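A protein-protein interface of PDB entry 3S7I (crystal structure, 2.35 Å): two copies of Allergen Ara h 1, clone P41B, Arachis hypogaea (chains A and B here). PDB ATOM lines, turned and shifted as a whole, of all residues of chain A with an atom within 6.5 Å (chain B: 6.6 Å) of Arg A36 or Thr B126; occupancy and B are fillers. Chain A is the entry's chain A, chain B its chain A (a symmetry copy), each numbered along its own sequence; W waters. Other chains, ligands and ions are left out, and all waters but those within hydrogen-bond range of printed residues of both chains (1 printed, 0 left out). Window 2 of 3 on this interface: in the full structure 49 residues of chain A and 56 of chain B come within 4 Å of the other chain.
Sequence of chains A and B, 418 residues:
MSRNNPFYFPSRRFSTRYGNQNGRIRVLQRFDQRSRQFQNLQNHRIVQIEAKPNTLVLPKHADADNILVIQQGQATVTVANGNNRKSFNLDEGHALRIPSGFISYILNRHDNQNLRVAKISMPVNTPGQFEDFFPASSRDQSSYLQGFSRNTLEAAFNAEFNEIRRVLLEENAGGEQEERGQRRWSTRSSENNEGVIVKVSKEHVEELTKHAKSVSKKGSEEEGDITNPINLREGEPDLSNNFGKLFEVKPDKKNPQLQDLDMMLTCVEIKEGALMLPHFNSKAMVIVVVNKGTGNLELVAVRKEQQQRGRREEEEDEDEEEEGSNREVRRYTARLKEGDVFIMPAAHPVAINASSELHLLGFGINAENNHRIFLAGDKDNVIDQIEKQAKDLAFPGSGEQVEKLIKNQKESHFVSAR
ND2 of Asn A40 is in hydrogen-bond range of O of Val B124, 2.9 Å away. O of Gln A37 lies close to O of Asn B125 (3.5 Å). The side-chain sulfur of Met A285 sits close to the backbone carbonyl oxygen of Val B124, at 3.5 Å. The side-chain amide oxygen (OD1) of Asn B125 sits close to the side-chain sulfur (SD) of Met A285. O of Asn B125 lies within hydrogen-bond range of ND2 of Asn A40, 3.3 Å away.
Printed residues of chain A within 4 Å of Asn B125: Gln A37 (3.5 Å), Asn A40 (3.3 Å) and Met A285 (3.4 Å). Printed residues of chain A within 4 Å of Pro B127: Asn A40 (3.9 Å). The nearest residue of chain A that does not touch Thr B126 is Phe A38 (5.1 Å).
Among the printed residues, pairs that only touch across the chains: Arg A36 with Thr B126, Gln A37 with Thr B126, Asn A40 with Thr B126 and Asn A40 with Pro B127.
Of the 10 printed residues of chain A, 4 touch a printed residue of chain B. Hydrophobic or aromatic side chains of chain A within 4 Å of the printed part of chain B: Met A285. Among the printed residues, no Asp or Glu carboxylate lies within 4 Å of a Lys or Arg side-chain nitrogen of the other chain.
The side-chain hydroxyl (OG) of Ser A35 sits at hydrogen-bond distance from the side-chain amide oxygen (OE1) of Gln A37 (3.3 Å). O of Asp B63 sits at hydrogen-bond distance from N of Val B124 (3.1 Å). The side-chain amide nitrogen of Asn B125 is in hydrogen-bond range of the side-chain carboxylate of Asp B63 (3.1 Å).
Water W1 lies within hydrogen-bond range of the side-chain amide nitrogen of Asn A40, the backbone carbonyl oxygen of Pro B123 and the side-chain amide nitrogen of Asn B43.
No position is printed for both chains.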
ATOM      1  N   PHE A  31     -11.172  21.337  11.260  1.00  0.00           N
ATOM      2  CA  PHE A  31      -9.816  20.790  11.011  1.00  0.00           C
ATOM      3  C   PHE A  31      -9.309  21.019   9.618  1.00  0.00           C
ATOM      4  O   PHE A  31      -8.070  21.043   9.425  1.00  0.00           O
ATOM      5  CB  PHE A  31      -9.790  19.302  11.214  1.00  0.00           C
ATOM      6  CG  PHE A  31      -9.848  18.881  12.658  1.00  0.00           C
ATOM      7  CD1 PHE A  31      -8.840  19.212  13.530  1.00  0.00           C
ATOM      8  CD2 PHE A  31     -10.884  18.092  13.113  1.00  0.00           C
ATOM      9  CE1 PHE A  31      -8.877  18.786  14.869  1.00  0.00           C
ATOM     10  CE2 PHE A  31     -10.911  17.651  14.417  1.00  0.00           C
ATOM     11  CZ  PHE A  31      -9.890  18.004  15.294  1.00  0.00           C
ATOM     12  N   ASP A  32     -10.238  21.164   8.656  1.00  0.00           N
ATOM     13  CA  ASP A  32      -9.865  21.420   7.282  1.00  0.00           C
ATOM     14  C   ASP A  32      -9.737  22.893   6.967  1.00  0.00           C
ATOM     15  O   ASP A  32      -9.480  23.277   5.827  1.00  0.00           O
ATOM     16  CB  ASP A  32     -10.818  20.740   6.302  1.00  0.00           C
ATOM     17  CG  ASP A  32     -12.248  21.237   6.406  1.00  0.00           C
ATOM     18  OD1 ASP A  32     -12.937  21.190   5.378  1.00  0.00           O
ATOM     19  OD2 ASP A  32     -12.715  21.650   7.472  1.00  0.00           O
ATOM     20  N   ARG A  34      -7.579  24.322   8.676  1.00  0.00           N
ATOM     21  CA  ARG A  34      -6.142  24.168   8.844  1.00  0.00           C
ATOM     22  C   ARG A  34      -5.511  23.813   7.510  1.00  0.00           C
ATOM     23  O   ARG A  34      -4.821  24.656   6.897  1.00  0.00           O
ATOM     24  CB  ARG A  34      -5.835  23.049   9.863  1.00  0.00           C
ATOM     25  CG  ARG A  34      -4.380  23.062  10.392  1.00  0.00           C
ATOM     26  CD  ARG A  34      -4.269  24.049  11.594  1.00  0.00           C
ATOM     27  NE  ARG A  34      -2.942  24.645  11.801  1.00  0.00           N
ATOM     28  CZ  ARG A  34      -2.104  24.314  12.792  1.00  0.00           C
ATOM     29  NH1 ARG A  34      -0.927  24.954  12.898  1.00  0.00           N
ATOM     30  NH2 ARG A  34      -2.418  23.346  13.670  1.00  0.00           N
ATOM     31  N   SER A  35      -5.815  22.589   7.044  1.00  0.00           N
ATOM     32  CA  SER A  35      -4.965  21.831   6.125  1.00  0.00           C
ATOM     33  C   SER A  35      -5.841  20.837   5.331  1.00  0.00           C
ATOM     34  O   SER A  35      -6.842  20.308   5.862  1.00  0.00           O
ATOM     35  CB  SER A  35      -3.891  21.094   6.969  1.00  0.00           C
ATOM     36  OG  SER A  35      -2.985  20.278   6.215  1.00  0.00           O
ATOM     37  N   ARG A  36      -5.493  20.585   4.067  1.00  0.00           N
ATOM     38  CA  ARG A  36      -6.284  19.689   3.220  1.00  0.00           C
ATOM     39  C   ARG A  36      -6.036  18.240   3.647  1.00  0.00           C
ATOM     40  O   ARG A  36      -6.827  17.343   3.332  1.00  0.00           O
ATOM     41  CB  ARG A  36      -5.974  19.888   1.735  1.00  0.00           C
ATOM     42  N   GLN A  37      -4.964  18.016   4.396  1.00  0.00           N
ATOM     43  CA  GLN A  37      -4.726  16.727   5.059  1.00  0.00           C
ATOM     44  C   GLN A  37      -5.856  16.282   5.963  1.00  0.00           C
ATOM     45  O   GLN A  37      -5.875  15.122   6.443  1.00  0.00           O
ATOM     46  CB  GLN A  37      -3.492  16.843   5.948  1.00  0.00           C
ATOM     47  CG  GLN A  37      -2.254  16.713   5.197  1.00  0.00           C
ATOM     48  CD  GLN A  37      -1.062  16.909   6.080  1.00  0.00           C
ATOM     49  OE1 GLN A  37      -0.598  18.050   6.292  1.00  0.00           O
ATOM     50  NE2 GLN A  37      -0.550  15.799   6.619  1.00  0.00           N
ATOM     51  N   PHE A  38      -6.722  17.201   6.335  1.00  0.00           N
ATOM     52  CA  PHE A  38      -7.721  16.833   7.358  1.00  0.00           C
ATOM     53  C   PHE A  38      -9.112  16.897   6.752  1.00  0.00           C
ATOM     54  O   PHE A  38     -10.101  17.073   7.434  1.00  0.00           O
ATOM     55  CB  PHE A  38      -7.533  17.684   8.644  1.00  0.00           C
ATOM     56  CG  PHE A  38      -6.139  17.529   9.264  1.00  0.00           C
ATOM     57  CD1 PHE A  38      -5.561  16.277   9.398  1.00  0.00           C
ATOM     58  CD2 PHE A  38      -5.371  18.651   9.582  1.00  0.00           C
ATOM     59  CE1 PHE A  38      -4.248  16.157   9.855  1.00  0.00           C
ATOM     60  CE2 PHE A  38      -4.103  18.542  10.033  1.00  0.00           C
ATOM     61  CZ  PHE A  38      -3.528  17.305  10.195  1.00  0.00           C
ATOM     62  N   GLN A  39      -9.190  16.728   5.448  1.00  0.00           N
ATOM     63  CA  GLN A  39     -10.487  16.675   4.844  1.00  0.00           C
ATOM     64  C   GLN A  39     -11.290  15.526   5.474  1.00  0.00           C
ATOM     65  O   GLN A  39     -12.434  15.697   5.750  1.00  0.00           O
ATOM     66  CB  GLN A  39     -10.382  16.604   3.334  1.00  0.00           C
ATOM     67  CG  GLN A  39     -11.744  16.664   2.649  1.00  0.00           C
ATOM     68  CD  GLN A  39     -12.486  17.996   2.907  1.00  0.00           C
ATOM     69  OE1 GLN A  39     -13.652  18.003   3.381  1.00  0.00           O
ATOM     70  NE2 GLN A  39     -11.805  19.141   2.618  1.00  0.00           N
ATOM     71  N   ASN A  40     -10.686  14.389   5.724  1.00  0.00           N
ATOM     72  CA  ASN A  40     -11.431  13.255   6.218  1.00  0.00           C
ATOM     73  C   ASN A  40     -11.884  13.470   7.625  1.00  0.00           C
ATOM     74  O   ASN A  40     -12.789  12.786   8.109  1.00  0.00           O
ATOM     75  CB  ASN A  40     -10.636  11.935   6.092  1.00  0.00           C
ATOM     76  CG  ASN A  40     -10.738  11.345   4.677  1.00  0.00           C
ATOM     77  OD1 ASN A  40     -11.596  11.750   3.927  1.00  0.00           O
ATOM     78  ND2 ASN A  40      -9.878  10.432   4.324  1.00  0.00           N
ATOM     79  N   MET A 285      -8.042   6.995  12.117  1.00  0.00           N
ATOM     80  CA  MET A 285      -7.556   8.364  12.330  1.00  0.00           C
ATOM     81  C   MET A 285      -8.102   8.796  13.666  1.00  0.00           C
ATOM     82  O   MET A 285      -9.324   8.704  13.906  1.00  0.00           O
ATOM     83  CB  MET A 285      -8.165   9.287  11.303  1.00  0.00           C
ATOM     84  CG  MET A 285      -7.888   8.875   9.907  1.00  0.00           C
ATOM     85  SD  MET A 285      -8.538  10.047   8.774  1.00  0.00           S
ATOM     86  CE  MET A 285     -10.027   9.117   8.512  1.00  0.00           C
ATOM     87  N   ARG B  30      -4.071  11.234 -10.060  1.00  0.00           N
ATOM     88  CA  ARG B  30      -5.355  11.255  -9.402  1.00  0.00           C
ATOM     89  C   ARG B  30      -6.410  11.486 -10.438  1.00  0.00           C
ATOM     90  O   ARG B  30      -6.287  12.392 -11.247  1.00  0.00           O
ATOM     91  CB  ARG B  30      -5.438  12.385  -8.401  1.00  0.00           C
ATOM     92  CG  ARG B  30      -4.725  12.124  -7.142  1.00  0.00           C
ATOM     93  CD  ARG B  30      -4.893  13.267  -6.120  1.00  0.00           C
ATOM     94  NE  ARG B  30      -6.307  13.666  -6.000  1.00  0.00           N
ATOM     95  CZ  ARG B  30      -6.764  14.609  -5.171  1.00  0.00           C
ATOM     96  NH1 ARG B  30      -8.072  14.901  -5.189  1.00  0.00           N
ATOM     97  NH2 ARG B  30      -5.949  15.254  -4.330  1.00  0.00           N
ATOM     98  N   ASN B  43     -10.706   8.640  -4.588  1.00  0.00           N
ATOM     99  CA  ASN B  43      -9.996   7.935  -3.563  1.00  0.00           C
ATOM    100  C   ASN B  43      -9.389   6.633  -4.005  1.00  0.00           C
ATOM    101  O   ASN B  43      -9.051   5.838  -3.190  1.00  0.00           O
ATOM    102  CB  ASN B  43     -10.797   7.750  -2.260  1.00  0.00           C
ATOM    103  CG  ASN B  43      -9.816   7.559  -1.064  1.00  0.00           C
ATOM    104  OD1 ASN B  43      -8.878   8.327  -0.954  1.00  0.00           O
ATOM    105  ND2 ASN B  43      -9.988   6.509  -0.256  1.00  0.00           N
ATOM    106  N   ASP B  63      -0.455   4.253   4.093  1.00  0.00           N
ATOM    107  CA  ASP B  63      -1.658   4.701   4.748  1.00  0.00           C
ATOM    108  C   ASP B  63      -2.835   4.651   3.774  1.00  0.00           C
ATOM    109  O   ASP B  63      -3.553   5.583   3.602  1.00  0.00           O
ATOM    110  CB  ASP B  63      -1.459   6.085   5.362  1.00  0.00           C
ATOM    111  CG  ASP B  63      -1.093   7.126   4.352  1.00  0.00           C
ATOM    112  OD1 ASP B  63      -1.342   8.285   4.597  1.00  0.00           O
ATOM    113  OD2 ASP B  63      -0.578   6.789   3.310  1.00  0.00           O
ATOM    114  N   PRO B 123      -6.539   5.509  -0.173  1.00  0.00           N
ATOM    115  CA  PRO B 123      -6.034   6.291   0.935  1.00  0.00           C
ATOM    116  C   PRO B 123      -7.000   6.469   2.048  1.00  0.00           C
ATOM    117  O   PRO B 123      -8.164   6.640   1.835  1.00  0.00           O
ATOM    118  CB  PRO B 123      -5.776   7.643   0.294  1.00  0.00           C
ATOM    119  CG  PRO B 123      -5.460   7.265  -1.173  1.00  0.00           C
ATOM    120  CD  PRO B 123      -6.344   6.194  -1.464  1.00  0.00           C
ATOM    121  N   VAL B 124      -6.453   6.586   3.223  1.00  0.00           N
ATOM    122  CA  VAL B 124      -7.213   6.696   4.443  1.00  0.00           C
ATOM    123  C   VAL B 124      -7.187   8.100   5.059  1.00  0.00           C
ATOM    124  O   VAL B 124      -8.164   8.573   5.656  1.00  0.00           O
ATOM    125  CB  VAL B 124      -6.591   5.757   5.519  1.00  0.00           C
ATOM    126  CG1 VAL B 124      -7.317   6.045   6.841  1.00  0.00           C
ATOM    127  CG2 VAL B 124      -6.777   4.283   5.072  1.00  0.00           C
ATOM    128  N   ASN B 125      -6.071   8.790   4.935  1.00  0.00           N
ATOM    129  CA  ASN B 125      -6.000  10.101   5.578  1.00  0.00           C
ATOM    130  C   ASN B 125      -6.516  11.271   4.756  1.00  0.00           C
ATOM    131  O   ASN B 125      -7.236  12.138   5.253  1.00  0.00           O
ATOM    132  CB  ASN B 125      -4.602  10.314   6.057  1.00  0.00           C
ATOM    133  CG  ASN B 125      -4.233   9.348   7.171  1.00  0.00           C
ATOM    134  OD1 ASN B 125      -4.986   9.196   8.111  1.00  0.00           O
ATOM    135  ND2 ASN B 125      -3.150   8.655   7.039  1.00  0.00           N
ATOM    136  N   THR B 126      -6.159  11.291   3.483  1.00  0.00           N
ATOM    137  CA  THR B 126      -6.415  12.445   2.612  1.00  0.00           C
ATOM    138  C   THR B 126      -6.892  11.939   1.285  1.00  0.00           C
ATOM    139  O   THR B 126      -6.197  11.122   0.664  1.00  0.00           O
ATOM    140  CB  THR B 126      -5.116  13.217   2.344  1.00  0.00           C
ATOM    141  OG1 THR B 126      -4.486  13.506   3.581  1.00  0.00           O
ATOM    142  CG2 THR B 126      -5.427  14.530   1.620  1.00  0.00           C
ATOM    143  N   PRO B 127      -8.066  12.386   0.836  1.00  0.00           N
ATOM    144  CA  PRO B 127      -8.632  11.701  -0.351  1.00  0.00           C
ATOM    145  C   PRO B 127      -7.684  11.683  -1.518  1.00  0.00           C
ATOM    146  O   PRO B 127      -7.196  12.723  -1.913  1.00  0.00           O
ATOM    147  CB  PRO B 127      -9.862  12.557  -0.691  1.00  0.00           C
ATOM    148  CG  PRO B 127     -10.287  13.090   0.533  1.00  0.00           C
ATOM    149  CD  PRO B 127      -8.998  13.370   1.371  1.00  0.00           C
ATOM    150  N   GLY B 128      -7.446  10.538  -2.096  1.00  0.00           N
ATOM    151  CA  GLY B 128      -6.597  10.445  -3.314  1.00  0.00           C
ATOM    152  C   GLY B 128      -5.055  10.558  -3.137  1.00  0.00           C
ATOM    153  O   GLY B 128      -4.334  10.602  -4.122  1.00  0.00           O
ATOM    154  N   GLN B 129      -4.578  10.596  -1.911  1.00  0.00           N
ATOM    155  CA  GLN B 129      -3.162  10.719  -1.614  1.00  0.00           C
ATOM    156  C   GLN B 129      -2.727   9.813  -0.519  1.00  0.00           C
ATOM    157  O   GLN B 129      -3.398   9.706   0.451  1.00  0.00           O
ATOM    158  CB  GLN B 129      -2.790  12.131  -1.229  1.00  0.00           C
ATOM    159  CG  GLN B 129      -2.293  12.909  -2.439  1.00  0.00           C
ATOM    160  CD  GLN B 129      -2.177  14.384  -2.114  1.00  0.00           C
ATOM    161  OE1 GLN B 129      -1.061  14.903  -1.986  1.00  0.00           O
ATOM    162  NE2 GLN B 129      -3.323  15.053  -1.923  1.00  0.00           N
ATOM    163  N   PHE B 130      -1.618   9.138  -0.738  1.00  0.00           N
ATOM    164  CA  PHE B 130      -1.012   8.239   0.208  1.00  0.00           C
ATOM    165  C   PHE B 130       0.524   8.250   0.051  1.00  0.00           C
ATOM    166  O   PHE B 130       1.069   8.668  -0.958  1.00  0.00           O
ATOM    167  CB  PHE B 130      -1.562   6.827   0.032  1.00  0.00           C
ATOM    168  CG  PHE B 130      -1.094   6.155  -1.226  1.00  0.00           C
ATOM    169  CD1 PHE B 130      -0.013   5.302  -1.211  1.00  0.00           C
ATOM    170  CD2 PHE B 130      -1.768   6.328  -2.428  1.00  0.00           C
ATOM    171  CE1 PHE B 130       0.416   4.703  -2.353  1.00  0.00           C
ATOM    172  CE2 PHE B 130      -1.319   5.686  -3.573  1.00  0.00           C
ATOM    173  CZ  PHE B 130      -0.212   4.927  -3.529  1.00  0.00           C
HETATM  174  O   HOH W   1     -10.397   8.930   2.071  1.00  0.00           O
